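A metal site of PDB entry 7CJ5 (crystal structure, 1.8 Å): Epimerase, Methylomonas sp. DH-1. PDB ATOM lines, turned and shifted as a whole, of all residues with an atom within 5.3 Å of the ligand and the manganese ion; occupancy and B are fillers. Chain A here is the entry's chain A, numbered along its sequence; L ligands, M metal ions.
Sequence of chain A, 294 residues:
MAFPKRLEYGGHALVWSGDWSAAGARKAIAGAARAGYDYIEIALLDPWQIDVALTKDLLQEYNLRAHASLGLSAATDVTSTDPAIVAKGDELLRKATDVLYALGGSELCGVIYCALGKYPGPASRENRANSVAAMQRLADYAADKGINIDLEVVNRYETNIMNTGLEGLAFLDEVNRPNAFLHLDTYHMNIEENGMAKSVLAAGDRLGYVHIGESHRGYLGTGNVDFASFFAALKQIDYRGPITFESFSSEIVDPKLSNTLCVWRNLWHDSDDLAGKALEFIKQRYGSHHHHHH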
ATOM      1  N   HIS A  12       7.948  29.852 -14.247  1.00  0.00           N
ATOM      2  CA  HIS A  12       7.792  28.866 -15.340  1.00  0.00           C
ATOM      3  C   HIS A  12       6.978  27.684 -14.816  1.00  0.00           C
ATOM      4  O   HIS A  12       7.361  27.126 -13.768  1.00  0.00           O
ATOM      5  CB  HIS A  12       9.151  28.433 -15.892  1.00  0.00           C
ATOM      6  CG  HIS A  12       9.065  27.834 -17.252  1.00  0.00           C
ATOM      7  ND1 HIS A  12       8.426  26.627 -17.481  1.00  0.00           N
ATOM      8  CD2 HIS A  12       9.533  28.248 -18.450  1.00  0.00           C
ATOM      9  CE1 HIS A  12       8.517  26.321 -18.755  1.00  0.00           C
ATOM     10  NE2 HIS A  12       9.188  27.306 -19.385  1.00  0.00           N
ATOM     11  N   LEU A  14       6.886  24.733 -15.570  1.00  0.00           N
ATOM     12  CA  LEU A  14       7.624  23.441 -15.521  1.00  0.00           C
ATOM     13  C   LEU A  14       8.428  23.360 -14.228  1.00  0.00           C
ATOM     14  O   LEU A  14       8.904  22.266 -13.932  1.00  0.00           O
ATOM     15  CB  LEU A  14       8.542  23.313 -16.743  1.00  0.00           C
ATOM     16  CG  LEU A  14       7.845  23.209 -18.095  1.00  0.00           C
ATOM     17  CD1 LEU A  14       8.852  22.818 -19.165  1.00  0.00           C
ATOM     18  CD2 LEU A  14       6.687  22.223 -18.065  1.00  0.00           C
ATOM     19  N   GLU A  41       4.171  31.401 -16.625  1.00  0.00           N
ATOM     20  CA  GLU A  41       4.577  31.137 -18.027  1.00  0.00           C
ATOM     21  C   GLU A  41       4.207  29.684 -18.333  1.00  0.00           C
ATOM     22  O   GLU A  41       4.844  28.758 -17.795  1.00  0.00           O
ATOM     23  CB  GLU A  41       6.055  31.412 -18.220  1.00  0.00           C
ATOM     24  CG  GLU A  41       6.489  31.264 -19.664  1.00  0.00           C
ATOM     25  CD  GLU A  41       7.942  31.589 -19.891  1.00  0.00           C
ATOM     26  OE1 GLU A  41       8.368  32.661 -19.440  1.00  0.00           O
ATOM     27  OE2 GLU A  41       8.660  30.761 -20.491  1.00  0.00           O
ATOM     28  N   ALA A  43       3.927  26.335 -20.472  1.00  0.00           N
ATOM     29  CA  ALA A  43       4.702  25.642 -21.520  1.00  0.00           C
ATOM     30  C   ALA A  43       3.713  25.028 -22.508  1.00  0.00           C
ATOM     31  O   ALA A  43       2.900  24.200 -22.099  1.00  0.00           O
ATOM     32  CB  ALA A  43       5.603  24.609 -20.885  1.00  0.00           C
ATOM     33  N   LEU A  45       4.319  23.311 -25.433  1.00  0.00           N
ATOM     34  CA  LEU A  45       5.057  22.404 -26.365  1.00  0.00           C
ATOM     35  C   LEU A  45       4.031  21.578 -27.146  1.00  0.00           C
ATOM     36  O   LEU A  45       4.310  21.254 -28.328  1.00  0.00           O
ATOM     37  CB  LEU A  45       6.036  21.530 -25.584  1.00  0.00           C
ATOM     38  CG  LEU A  45       7.447  22.113 -25.440  1.00  0.00           C
ATOM     39  CD1 LEU A  45       7.484  23.198 -24.379  1.00  0.00           C
ATOM     40  CD2 LEU A  45       8.469  21.019 -25.144  1.00  0.00           C
ATOM     41  N   SER A  69       5.359  30.089 -23.346  1.00  0.00           N
ATOM     42  CA  SER A  69       6.603  29.771 -24.081  1.00  0.00           C
ATOM     43  C   SER A  69       6.472  28.362 -24.650  1.00  0.00           C
ATOM     44  O   SER A  69       5.645  27.559 -24.141  1.00  0.00           O
ATOM     45  CB  SER A  69       7.821  29.897 -23.194  1.00  0.00           C
ATOM     46  OG  SER A  69       7.765  28.983 -22.117  1.00  0.00           O
ATOM     47  N   LEU A  70       7.251  28.072 -25.667  1.00  0.00           N
ATOM     48  CA  LEU A  70       7.379  26.681 -26.148  1.00  0.00           C
ATOM     49  C   LEU A  70       8.696  26.580 -26.906  1.00  0.00           C
ATOM     50  O   LEU A  70       9.284  27.629 -27.235  1.00  0.00           O
ATOM     51  CB  LEU A  70       6.187  26.331 -27.038  1.00  0.00           C
ATOM     52  CG  LEU A  70       6.013  27.203 -28.283  1.00  0.00           C
ATOM     53  CD1 LEU A  70       6.829  26.654 -29.439  1.00  0.00           C
ATOM     54  CD2 LEU A  70       4.555  27.310 -28.660  1.00  0.00           C
ATOM     55  N   GLY A  71       9.129  25.341 -27.118  1.00  0.00           N
ATOM     56  CA  GLY A  71      10.131  24.972 -28.118  1.00  0.00           C
ATOM     57  C   GLY A  71       9.501  24.038 -29.134  1.00  0.00           C
ATOM     58  O   GLY A  71       8.714  23.160 -28.725  1.00  0.00           O
ATOM     59  N   CYS A 109       6.730  33.523 -26.125  1.00  0.00           N
ATOM     60  CA  CYS A 109       8.212  33.597 -26.146  1.00  0.00           C
ATOM     61  C   CYS A 109       8.798  32.183 -26.192  1.00  0.00           C
ATOM     62  O   CYS A 109       8.040  31.203 -26.316  1.00  0.00           O
ATOM     63  CB  CYS A 109       8.732  34.368 -24.946  1.00  0.00           C
ATOM     64  SG  CYS A 109       8.375  33.555 -23.368  1.00  0.00           S
ATOM     65  N   GLY A 110      10.124  32.110 -26.069  1.00  0.00           N
ATOM     66  CA  GLY A 110      10.859  30.840 -26.084  1.00  0.00           C
ATOM     67  C   GLY A 110      11.400  30.509 -27.462  1.00  0.00           C
ATOM     68  O   GLY A 110      11.576  31.438 -28.293  1.00  0.00           O
ATOM     69  N   VAL A 111      11.687  29.229 -27.693  1.00  0.00           N
ATOM     70  CA  VAL A 111      12.348  28.754 -28.936  1.00  0.00           C
ATOM     71  C   VAL A 111      11.235  28.442 -29.938  1.00  0.00           C
ATOM     72  O   VAL A 111      10.960  27.257 -30.211  1.00  0.00           O
ATOM     73  CB  VAL A 111      13.319  27.595 -28.632  1.00  0.00           C
ATOM     74  CG1 VAL A 111      14.127  27.184 -29.863  1.00  0.00           C
ATOM     75  CG2 VAL A 111      14.263  27.967 -27.503  1.00  0.00           C
ATOM     76  N   LEU A 116      13.924  22.989 -30.559  1.00  0.00           N
ATOM     77  CA  LEU A 116      14.762  23.089 -29.346  1.00  0.00           C
ATOM     78  C   LEU A 116      15.630  21.830 -29.243  1.00  0.00           C
ATOM     79  O   LEU A 116      15.075  20.733 -29.121  1.00  0.00           O
ATOM     80  CB  LEU A 116      13.858  23.233 -28.115  1.00  0.00           C
ATOM     81  CG  LEU A 116      14.585  23.256 -26.777  1.00  0.00           C
ATOM     82  CD1 LEU A 116      15.429  24.523 -26.667  1.00  0.00           C
ATOM     83  CD2 LEU A 116      13.602  23.163 -25.620  1.00  0.00           C
ATOM     84  N   GLU A 152      13.576  33.721 -28.173  1.00  0.00           N
ATOM     85  CA  GLU A 152      14.528  33.395 -27.087  1.00  0.00           C
ATOM     86  C   GLU A 152      15.856  32.930 -27.682  1.00  0.00           C
ATOM     87  O   GLU A 152      15.906  31.823 -28.228  1.00  0.00           O
ATOM     88  CB  GLU A 152      13.997  32.324 -26.157  1.00  0.00           C
ATOM     89  CG  GLU A 152      14.825  32.224 -24.890  1.00  0.00           C
ATOM     90  CD  GLU A 152      14.411  31.140 -23.920  1.00  0.00           C
ATOM     91  OE1 GLU A 152      13.434  30.429 -24.208  1.00  0.00           O
ATOM     92  OE2 GLU A 152      15.066  31.015 -22.859  1.00  0.00           O
ATOM     93  N   VAL A 154      19.143  31.112 -27.436  1.00  0.00           N
ATOM     94  CA  VAL A 154      19.606  29.993 -26.570  1.00  0.00           C
ATOM     95  C   VAL A 154      20.986  29.547 -27.037  1.00  0.00           C
ATOM     96  O   VAL A 154      21.441  29.972 -28.127  1.00  0.00           O
ATOM     97  CB  VAL A 154      18.586  28.839 -26.479  1.00  0.00           C
ATOM     98  CG1 VAL A 154      17.273  29.335 -25.860  1.00  0.00           C
ATOM     99  CG2 VAL A 154      18.316  28.150 -27.807  1.00  0.00           C
ATOM    100  N   GLU A 158      21.302  24.083 -28.058  1.00  0.00           N
ATOM    101  CA  GLU A 158      19.818  24.127 -28.058  1.00  0.00           C
ATOM    102  C   GLU A 158      19.265  24.812 -29.313  1.00  0.00           C
ATOM    103  O   GLU A 158      18.048  24.645 -29.560  1.00  0.00           O
ATOM    104  CB  GLU A 158      19.312  24.781 -26.763  1.00  0.00           C
ATOM    105  CG  GLU A 158      19.659  23.964 -25.529  1.00  0.00           C
ATOM    106  CD  GLU A 158      18.962  24.429 -24.259  1.00  0.00           C
ATOM    107  OE1 GLU A 158      17.884  25.057 -24.388  1.00  0.00           O
ATOM    108  OE2 GLU A 158      19.501  24.193 -23.162  1.00  0.00           O
ATOM    109  N   HIS A 183      14.248  38.011 -26.787  1.00  0.00           N
ATOM    110  CA  HIS A 183      14.093  37.341 -25.480  1.00  0.00           C
ATOM    111  C   HIS A 183      15.479  36.836 -25.063  1.00  0.00           C
ATOM    112  O   HIS A 183      16.097  36.084 -25.837  1.00  0.00           O
ATOM    113  CB  HIS A 183      12.975  36.310 -25.608  1.00  0.00           C
ATOM    114  CG  HIS A 183      12.779  35.407 -24.446  1.00  0.00           C
ATOM    115  ND1 HIS A 183      11.910  34.334 -24.494  1.00  0.00           N
ATOM    116  CD2 HIS A 183      13.356  35.379 -23.221  1.00  0.00           C
ATOM    117  CE1 HIS A 183      11.939  33.698 -23.342  1.00  0.00           C
ATOM    118  NE2 HIS A 183      12.832  34.325 -22.540  1.00  0.00           N
ATOM    119  N   ASP A 185      18.041  35.155 -21.931  1.00  0.00           N
ATOM    120  CA  ASP A 185      18.025  34.150 -20.844  1.00  0.00           C
ATOM    121  C   ASP A 185      19.428  34.088 -20.236  1.00  0.00           C
ATOM    122  O   ASP A 185      20.362  33.751 -20.982  1.00  0.00           O
ATOM    123  CB  ASP A 185      17.592  32.789 -21.404  1.00  0.00           C
ATOM    124  CG  ASP A 185      17.530  31.690 -20.357  1.00  0.00           C
ATOM    125  OD1 ASP A 185      18.401  31.685 -19.475  1.00  0.00           O
ATOM    126  OD2 ASP A 185      16.608  30.843 -20.448  1.00  0.00           O
ATOM    127  N   TYR A 187      21.015  32.090 -18.336  1.00  0.00           N
ATOM    128  CA  TYR A 187      21.688  30.757 -18.404  1.00  0.00           C
ATOM    129  C   TYR A 187      22.405  30.631 -19.760  1.00  0.00           C
ATOM    130  O   TYR A 187      23.586  30.233 -19.815  1.00  0.00           O
ATOM    131  CB  TYR A 187      20.682  29.627 -18.201  1.00  0.00           C
ATOM    132  CG  TYR A 187      21.169  28.263 -18.638  1.00  0.00           C
ATOM    133  CD1 TYR A 187      22.043  27.526 -17.853  1.00  0.00           C
ATOM    134  CD2 TYR A 187      20.755  27.725 -19.842  1.00  0.00           C
ATOM    135  CE1 TYR A 187      22.480  26.263 -18.258  1.00  0.00           C
ATOM    136  CE2 TYR A 187      21.194  26.479 -20.265  1.00  0.00           C
ATOM    137  CZ  TYR A 187      22.051  25.742 -19.466  1.00  0.00           C
ATOM    138  OH  TYR A 187      22.482  24.515 -19.876  1.00  0.00           O
ATOM    139  N   HIS A 188      21.703  30.969 -20.831  1.00  0.00           N
ATOM    140  CA  HIS A 188      22.245  30.914 -22.218  1.00  0.00           C
ATOM    141  C   HIS A 188      23.314  32.004 -22.389  1.00  0.00           C
ATOM    142  O   HIS A 188      24.376  31.716 -22.966  1.00  0.00           O
ATOM    143  CB  HIS A 188      21.092  31.015 -23.218  1.00  0.00           C
ATOM    144  CG  HIS A 188      20.155  29.855 -23.114  1.00  0.00           C
ATOM    145  ND1 HIS A 188      20.590  28.547 -23.283  1.00  0.00           N
ATOM    146  CD2 HIS A 188      18.832  29.784 -22.842  1.00  0.00           C
ATOM    147  CE1 HIS A 188      19.569  27.716 -23.147  1.00  0.00           C
ATOM    148  NE2 HIS A 188      18.485  28.455 -22.854  1.00  0.00           N
ATOM    149  N   HIS A 211      14.338  35.640 -19.296  1.00  0.00           N
ATOM    150  CA  HIS A 211      14.425  34.439 -18.427  1.00  0.00           C
ATOM    151  C   HIS A 211      15.621  34.586 -17.489  1.00  0.00           C
ATOM    152  O   HIS A 211      16.718  34.947 -17.947  1.00  0.00           O
ATOM    153  CB  HIS A 211      14.531  33.159 -19.252  1.00  0.00           C
ATOM    154  CG  HIS A 211      13.214  32.681 -19.756  1.00  0.00           C
ATOM    155  ND1 HIS A 211      13.085  31.531 -20.481  1.00  0.00           N
ATOM    156  CD2 HIS A 211      11.967  33.197 -19.639  1.00  0.00           C
ATOM    157  CE1 HIS A 211      11.828  31.344 -20.796  1.00  0.00           C
ATOM    158  NE2 HIS A 211      11.113  32.369 -20.298  1.00  0.00           N
ATOM    159  N   ARG A 217      21.508  26.186 -13.687  1.00  0.00           N
ATOM    160  CA  ARG A 217      20.005  26.205 -13.633  1.00  0.00           C
ATOM    161  C   ARG A 217      19.482  25.797 -12.246  1.00  0.00           C
ATOM    162  O   ARG A 217      18.285  25.439 -12.134  1.00  0.00           O
ATOM    163  CB  ARG A 217      19.370  25.284 -14.683  1.00  0.00           C
ATOM    164  CG  ARG A 217      20.087  25.284 -16.024  1.00  0.00           C
ATOM    165  CD  ARG A 217      19.182  24.829 -17.163  1.00  0.00           C
ATOM    166  NE  ARG A 217      18.448  25.944 -17.728  1.00  0.00           N
ATOM    167  CZ  ARG A 217      17.952  25.980 -18.948  1.00  0.00           C
ATOM    168  NH1 ARG A 217      18.088  24.943 -19.742  1.00  0.00           N
ATOM    169  NH2 ARG A 217      17.324  27.061 -19.371  1.00  0.00           N
ATOM    170  N   GLU A 246      13.096  30.252 -14.191  1.00  0.00           N
ATOM    171  CA  GLU A 246      12.886  28.846 -14.604  1.00  0.00           C
ATOM    172  C   GLU A 246      14.058  27.960 -14.175  1.00  0.00           C
ATOM    173  O   GLU A 246      15.208  28.447 -14.046  1.00  0.00           O
ATOM    174  CB  GLU A 246      12.686  28.787 -16.114  1.00  0.00           C
ATOM    175  CG  GLU A 246      13.952  29.023 -16.890  1.00  0.00           C
ATOM    176  CD  GLU A 246      13.755  29.069 -18.388  1.00  0.00           C
ATOM    177  OE1 GLU A 246      12.653  28.736 -18.853  1.00  0.00           O
ATOM    178  OE2 GLU A 246      14.707  29.459 -19.071  1.00  0.00           O
ATOM    179  N   PHE A 248      14.593  23.180 -14.295  1.00  0.00           N
ATOM    180  CA  PHE A 248      14.027  21.958 -14.930  1.00  0.00           C
ATOM    181  C   PHE A 248      14.532  20.725 -14.181  1.00  0.00           C
ATOM    182  O   PHE A 248      15.677  20.339 -14.406  1.00  0.00           O
ATOM    183  CB  PHE A 248      14.414  21.944 -16.411  1.00  0.00           C
ATOM    184  CG  PHE A 248      13.945  23.180 -17.132  1.00  0.00           C
ATOM    185  CD1 PHE A 248      12.614  23.319 -17.478  1.00  0.00           C
ATOM    186  CD2 PHE A 248      14.810  24.224 -17.416  1.00  0.00           C
ATOM    187  CE1 PHE A 248      12.155  24.458 -18.115  1.00  0.00           C
ATOM    188  CE2 PHE A 248      14.353  25.372 -18.049  1.00  0.00           C
ATOM    189  CZ  PHE A 248      13.025  25.489 -18.399  1.00  0.00           C
ATOM    190  N   LEU A 261      17.464  18.977 -22.543  1.00  0.00           N
ATOM    191  CA  LEU A 261      18.174  20.003 -21.739  1.00  0.00           C
ATOM    192  C   LEU A 261      19.354  19.345 -20.990  1.00  0.00           C
ATOM    193  O   LEU A 261      20.128  20.086 -20.329  1.00  0.00           O
ATOM    194  CB  LEU A 261      17.182  20.644 -20.778  1.00  0.00           C
ATOM    195  CG  LEU A 261      16.054  21.423 -21.444  1.00  0.00           C
ATOM    196  CD1 LEU A 261      15.196  22.146 -20.416  1.00  0.00           C
ATOM    197  CD2 LEU A 261      16.606  22.409 -22.462  1.00  0.00           C
HETATM  198  C1  LIG L   1      15.495  26.007 -22.505  1.00  0.00           C
HETATM  199  C2  LIG L   1      14.957  27.315 -21.991  1.00  0.00           C
HETATM  200  C3  LIG L   1      13.468  27.437 -21.798  1.00  0.00           C
HETATM  201  C4  LIG L   1      12.884  26.885 -23.081  1.00  0.00           C
HETATM  202  C5  LIG L   1      11.379  26.611 -23.124  1.00  0.00           C
HETATM  203  C6  LIG L   1      10.619  26.826 -21.835  1.00  0.00           C
HETATM  204  O1  LIG L   1      16.890  25.891 -22.214  1.00  0.00           O
HETATM  205  O2  LIG L   1      15.727  28.231 -21.719  1.00  0.00           O
HETATM  206  O3  LIG L   1      13.088  28.804 -21.591  1.00  0.00           O
HETATM  207  O4  LIG L   1      13.257  27.823 -24.067  1.00  0.00           O
HETATM  208  O5  LIG L   1      10.802  27.341 -24.201  1.00  0.00           O
HETATM  209  O6  LIG L   1       9.235  26.467 -22.087  1.00  0.00           O
HETATM  210 MN    MN M   1      14.803  30.155 -21.059  1.00  0.00          MN
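Within 4 Å of the manganese ion: Glu 152, Asp 185, His 211 and Glu 246. The nearest printed residue that does not touch the manganese ion is Arg 217 (4.3 Å).
N of Gly 71 touches O5 of the ligand, at 3.9 Å. Gly 110 touches the ligand (CA to O5, 3.97 Å). CG2 of Val 111 touches O4 of the ligand, at 3.6 Å. Phe 248 touches the ligand (CZ to C3, 3.9 Å). Leu 261 touches the ligand. Hydrophobic or aromatic side chains that line the ligand: His 12, Val 111, His 188, His 211, Phe 248 and Leu 261. 15 residues have an atom within 4 Å of the ligand: His 12, Ser 69, Leu 70, Gly 71, Gly 110, Val 111, Glu 152, Glu 158, Asp 185, His 188, His 211, Arg 217, Glu 246, Phe 248 and Leu 261. The nearest printed residue that does not touch the ligand is Ala 43 (4.3 Å).
NH1 of Arg 217 is in salt-bridge range of OE2 of Glu 158, at 3.8 Å. O of Leu 70 sits at hydrogen-bond distance from N of Val 111, 2.9 Å away. A ring nitrogen (ND1) of His 183 lies within hydrogen-bond range of the backbone NH (N) of Gly 110 (3.3 Å). A ring nitrogen (NE2) of His 211 lies within hydrogen-bond range of the side-chain carboxylate (OE1) of Glu 41 (2.9 Å). ND1 of His 12 lies close to N of Leu 14, at 3.1 Å. The side-chain hydroxyl (OG) of Ser 69 lies within hydrogen-bond range of the side-chain carboxylate (OE2) of Glu 41, 2.6 Å away. The backbone NH (N) of Glu 152 lies within hydrogen-bond range of the backbone carbonyl oxygen (O) of Gly 110 (3.0 Å). OD2 of Asp 185 lies close to NH2 of Arg 217.
The manganese ion is bound by the side-chain carboxylate (OE2) of Glu 152 (2.0 Å), the side-chain carboxylate (OD2) of Asp 185 (2.0 Å), the side-chain carboxylate (OE2) of Glu 246 (2.1 Å), an oxygen (O2) of the ligand (2.2 Å), an oxygen (O3) of the ligand (2.2 Å) and a ring nitrogen (ND1) of His 211 (2.3 Å). The manganese ion has six donor atoms within binding distance.
The side-chain carboxylate (OE1) of Glu 158 sits at hydrogen-bond distance from an oxygen (O1) of the ligand. OG of Ser 69 lies within hydrogen-bond range of O6 of the ligand (2.9 Å). The backbone carbonyl oxygen (O) of Leu 70 is in hydrogen-bond range of an oxygen (O5) of the ligand (3.4 Å). The guanidinium group (NH1) of Arg 217 lies within hydrogen-bond range of an oxygen (O1) of the ligand (2.9 Å). A ring nitrogen (NE2) of His 12 is in hydrogen-bond range of an oxygen (O6) of the ligand, 2.8 Å away. An oxygen (O1) of the ligand lies within hydrogen-bond range of a ring nitrogen (NE2) of His 188, at 3.1 Å.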
